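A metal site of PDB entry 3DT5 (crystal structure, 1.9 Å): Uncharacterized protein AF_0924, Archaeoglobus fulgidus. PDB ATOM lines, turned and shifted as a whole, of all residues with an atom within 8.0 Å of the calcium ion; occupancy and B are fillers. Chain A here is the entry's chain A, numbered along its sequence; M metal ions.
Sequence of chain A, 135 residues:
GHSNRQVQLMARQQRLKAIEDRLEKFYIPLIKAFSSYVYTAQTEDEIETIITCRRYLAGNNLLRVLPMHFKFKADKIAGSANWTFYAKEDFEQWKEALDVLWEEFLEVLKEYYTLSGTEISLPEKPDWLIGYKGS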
ATOM      1  N   TYR A  39       0.976   6.441  11.570  1.00  0.00           N
ATOM      2  CA  TYR A  39       1.753   7.102  12.594  1.00  0.00           C
ATOM      3  C   TYR A  39       2.958   6.224  12.799  1.00  0.00           C
ATOM      4  O   TYR A  39       2.814   4.988  12.831  1.00  0.00           O
ATOM      5  CB  TYR A  39       0.978   7.204  13.929  1.00  0.00           C
ATOM      6  CG  TYR A  39       1.883   7.671  15.049  1.00  0.00           C
ATOM      7  CD1 TYR A  39       2.157   9.046  15.228  1.00  0.00           C
ATOM      8  CD2 TYR A  39       2.554   6.754  15.866  1.00  0.00           C
ATOM      9  CE1 TYR A  39       3.056   9.489  16.240  1.00  0.00           C
ATOM     10  CE2 TYR A  39       3.464   7.188  16.864  1.00  0.00           C
ATOM     11  CZ  TYR A  39       3.690   8.555  17.052  1.00  0.00           C
ATOM     12  OH  TYR A  39       4.589   8.989  18.010  1.00  0.00           O
ATOM     13  N   GLU A  44       6.146  12.825  14.135  1.00  0.00           N
ATOM     14  CA  GLU A  44       6.252  14.174  14.711  1.00  0.00           C
ATOM     15  C   GLU A  44       7.357  14.955  14.005  1.00  0.00           C
ATOM     16  O   GLU A  44       7.208  16.154  13.730  1.00  0.00           O
ATOM     17  CB  GLU A  44       6.551  14.086  16.213  1.00  0.00           C
ATOM     18  CG  GLU A  44       5.422  13.481  17.060  1.00  0.00           C
ATOM     19  CD  GLU A  44       5.494  13.908  18.531  1.00  0.00           C
ATOM     20  OE1 GLU A  44       6.356  14.758  18.898  1.00  0.00           O
ATOM     21  OE2 GLU A  44       4.691  13.412  19.360  1.00  0.00           O
ATOM     22  N   PHE A  70       5.630  22.004  16.789  1.00  0.00           N
ATOM     23  CA  PHE A  70       4.555  21.011  16.994  1.00  0.00           C
ATOM     24  C   PHE A  70       4.966  19.895  17.992  1.00  0.00           C
ATOM     25  O   PHE A  70       4.163  19.530  18.850  1.00  0.00           O
ATOM     26  CB  PHE A  70       4.149  20.349  15.665  1.00  0.00           C
ATOM     27  CG  PHE A  70       3.199  19.186  15.859  1.00  0.00           C
ATOM     28  CD1 PHE A  70       1.871  19.420  16.217  1.00  0.00           C
ATOM     29  CD2 PHE A  70       3.659  17.864  15.742  1.00  0.00           C
ATOM     30  CE1 PHE A  70       0.995  18.326  16.427  1.00  0.00           C
ATOM     31  CE2 PHE A  70       2.772  16.779  15.964  1.00  0.00           C
ATOM     32  CZ  PHE A  70       1.442  17.047  16.299  1.00  0.00           C
ATOM     33  N   LYS A  71       6.174  19.371  17.821  1.00  0.00           N
ATOM     34  CA  LYS A  71       6.672  18.192  18.535  1.00  0.00           C
ATOM     35  C   LYS A  71       6.373  18.192  20.026  1.00  0.00           C
ATOM     36  O   LYS A  71       5.957  17.186  20.589  1.00  0.00           O
ATOM     37  CB  LYS A  71       8.210  18.153  18.477  1.00  0.00           C
ATOM     38  CG  LYS A  71       8.802  17.490  17.298  1.00  0.00           C
ATOM     39  CD  LYS A  71      10.343  17.482  17.415  1.00  0.00           C
ATOM     40  CE  LYS A  71      10.844  16.562  18.521  1.00  0.00           C
ATOM     41  NZ  LYS A  71      11.568  15.334  17.999  1.00  0.00           N
ATOM     42  N   PHE A  72       6.703  19.310  20.687  1.00  0.00           N
ATOM     43  CA  PHE A  72       6.570  19.341  22.121  1.00  0.00           C
ATOM     44  C   PHE A  72       5.221  19.848  22.601  1.00  0.00           C
ATOM     45  O   PHE A  72       5.046  20.122  23.785  1.00  0.00           O
ATOM     46  CB  PHE A  72       7.768  20.085  22.719  1.00  0.00           C
ATOM     47  CG  PHE A  72       9.089  19.430  22.392  1.00  0.00           C
ATOM     48  CD1 PHE A  72       9.376  18.140  22.850  1.00  0.00           C
ATOM     49  CD2 PHE A  72      10.033  20.078  21.580  1.00  0.00           C
ATOM     50  CE1 PHE A  72      10.602  17.505  22.532  1.00  0.00           C
ATOM     51  CE2 PHE A  72      11.268  19.457  21.244  1.00  0.00           C
ATOM     52  CZ  PHE A  72      11.556  18.169  21.732  1.00  0.00           C
ATOM     53  N   LYS A  73       4.250  19.953  21.699  1.00  0.00           N
ATOM     54  CA  LYS A  73       2.922  20.447  22.042  1.00  0.00           C
ATOM     55  C   LYS A  73       1.908  19.340  22.096  1.00  0.00           C
ATOM     56  O   LYS A  73       0.797  19.540  22.593  1.00  0.00           O
ATOM     57  CB  LYS A  73       2.406  21.488  21.019  1.00  0.00           C
ATOM     58  CG  LYS A  73       3.354  22.631  20.629  1.00  0.00           C
ATOM     59  CD  LYS A  73       3.708  23.469  21.760  1.00  0.00           C
ATOM     60  CE  LYS A  73       3.742  24.916  21.277  1.00  0.00           C
ATOM     61  NZ  LYS A  73       5.116  25.395  21.255  1.00  0.00           N
ATOM     62  N   ALA A  74       2.258  18.160  21.590  1.00  0.00           N
ATOM     63  CA  ALA A  74       1.268  17.084  21.448  1.00  0.00           C
ATOM     64  C   ALA A  74       1.956  15.724  21.346  1.00  0.00           C
ATOM     65  O   ALA A  74       3.143  15.660  21.105  1.00  0.00           O
ATOM     66  CB  ALA A  74       0.401  17.336  20.191  1.00  0.00           C
ATOM     67  N   ASP A  75       1.191  14.648  21.564  1.00  0.00           N
ATOM     68  CA  ASP A  75       1.637  13.256  21.484  1.00  0.00           C
ATOM     69  C   ASP A  75       0.461  12.408  21.096  1.00  0.00           C
ATOM     70  O   ASP A  75      -0.679  12.758  21.418  1.00  0.00           O
ATOM     71  CB  ASP A  75       2.110  12.700  22.864  1.00  0.00           C
ATOM     72  CG  ASP A  75       3.451  13.240  23.295  1.00  0.00           C
ATOM     73  OD1 ASP A  75       4.394  13.212  22.473  1.00  0.00           O
ATOM     74  OD2 ASP A  75       3.602  13.598  24.479  1.00  0.00           O
ATOM     75  N   LYS A  76       0.729  11.264  20.465  1.00  0.00           N
ATOM     76  CA  LYS A  76      -0.276  10.169  20.368  1.00  0.00           C
ATOM     77  C   LYS A  76       0.015   9.197  21.551  1.00  0.00           C
ATOM     78  O   LYS A  76       1.138   8.738  21.724  1.00  0.00           O
ATOM     79  CB  LYS A  76      -0.158   9.410  19.023  1.00  0.00           C
ATOM     80  CG  LYS A  76      -0.570  10.306  17.862  1.00  0.00           C
ATOM     81  CD  LYS A  76      -1.140   9.514  16.706  1.00  0.00           C
ATOM     82  CE  LYS A  76      -1.403  10.428  15.454  1.00  0.00           C
ATOM     83  NZ  LYS A  76      -2.258   9.686  14.448  1.00  0.00           N
ATOM     84  N   TRP A  83      -4.089  13.052  18.087  1.00  0.00           N
ATOM     85  CA  TRP A  83      -3.027  13.855  18.660  1.00  0.00           C
ATOM     86  C   TRP A  83      -3.603  14.523  19.925  1.00  0.00           C
ATOM     87  O   TRP A  83      -4.607  15.206  19.865  1.00  0.00           O
ATOM     88  CB  TRP A  83      -2.566  14.947  17.673  1.00  0.00           C
ATOM     89  CG  TRP A  83      -1.817  14.412  16.482  1.00  0.00           C
ATOM     90  CD1 TRP A  83      -2.310  14.287  15.183  1.00  0.00           C
ATOM     91  CD2 TRP A  83      -0.487  13.924  16.465  1.00  0.00           C
ATOM     92  NE1 TRP A  83      -1.318  13.756  14.364  1.00  0.00           N
ATOM     93  CE2 TRP A  83      -0.187  13.554  15.128  1.00  0.00           C
ATOM     94  CE3 TRP A  83       0.525  13.805  17.457  1.00  0.00           C
ATOM     95  CZ2 TRP A  83       1.063  13.004  14.756  1.00  0.00           C
ATOM     96  CZ3 TRP A  83       1.788  13.300  17.066  1.00  0.00           C
ATOM     97  CH2 TRP A  83       2.032  12.916  15.734  1.00  0.00           C
ATOM     98  N   THR A  84      -2.965  14.271  21.073  1.00  0.00           N
ATOM     99  CA  THR A  84      -3.414  14.873  22.330  1.00  0.00           C
ATOM    100  C   THR A  84      -2.566  16.117  22.530  1.00  0.00           C
ATOM    101  O   THR A  84      -1.334  16.030  22.629  1.00  0.00           O
ATOM    102  CB  THR A  84      -3.177  13.931  23.534  1.00  0.00           C
ATOM    103  OG1 THR A  84      -4.077  12.824  23.418  1.00  0.00           O
ATOM    104  CG2 THR A  84      -3.481  14.654  24.892  1.00  0.00           C
ATOM    105  N   TYR A  86      -1.466  19.313  24.898  1.00  0.00           N
ATOM    106  CA  TYR A  86      -1.418  19.611  26.334  1.00  0.00           C
ATOM    107  C   TYR A  86      -2.005  20.967  26.691  1.00  0.00           C
ATOM    108  O   TYR A  86      -2.500  21.127  27.781  1.00  0.00           O
ATOM    109  CB  TYR A  86      -0.019  19.422  26.903  1.00  0.00           C
ATOM    110  CG  TYR A  86       0.445  17.998  26.696  1.00  0.00           C
ATOM    111  CD1 TYR A  86      -0.180  16.941  27.367  1.00  0.00           C
ATOM    112  CD2 TYR A  86       1.475  17.700  25.778  1.00  0.00           C
ATOM    113  CE1 TYR A  86       0.198  15.645  27.145  1.00  0.00           C
ATOM    114  CE2 TYR A  86       1.863  16.420  25.568  1.00  0.00           C
ATOM    115  CZ  TYR A  86       1.223  15.379  26.246  1.00  0.00           C
ATOM    116  OH  TYR A  86       1.657  14.055  26.033  1.00  0.00           O
HETATM  117 CA    CA M   1       5.345  14.994  21.193  1.00  0.00          CA
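The calcium ion is bound by O of Ala 74 (2.3 Å), O of Lys 71 (2.4 Å), OD1 of Asp 75 (2.4 Å), OE2 of Glu 44 (2.5 Å) and OE1 of Glu 44 (2.5 Å). The calcium ion has five donor atoms within binding distance.
Four residues have an atom within 4 Å of the calcium ion: Glu 44, Lys 71, Ala 74 and Asp 75. The nearest printed residue that does not touch the calcium ion is Phe 72 (4.6 Å).
The side-chain hydroxyl of Tyr 86 is in hydrogen-bond range of the side-chain carboxylate of Asp 75 (2.5 Å). The backbone NH (N) of Thr 84 sits at hydrogen-bond distance from the backbone carbonyl oxygen (O) of Asp 75 (2.8 Å).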
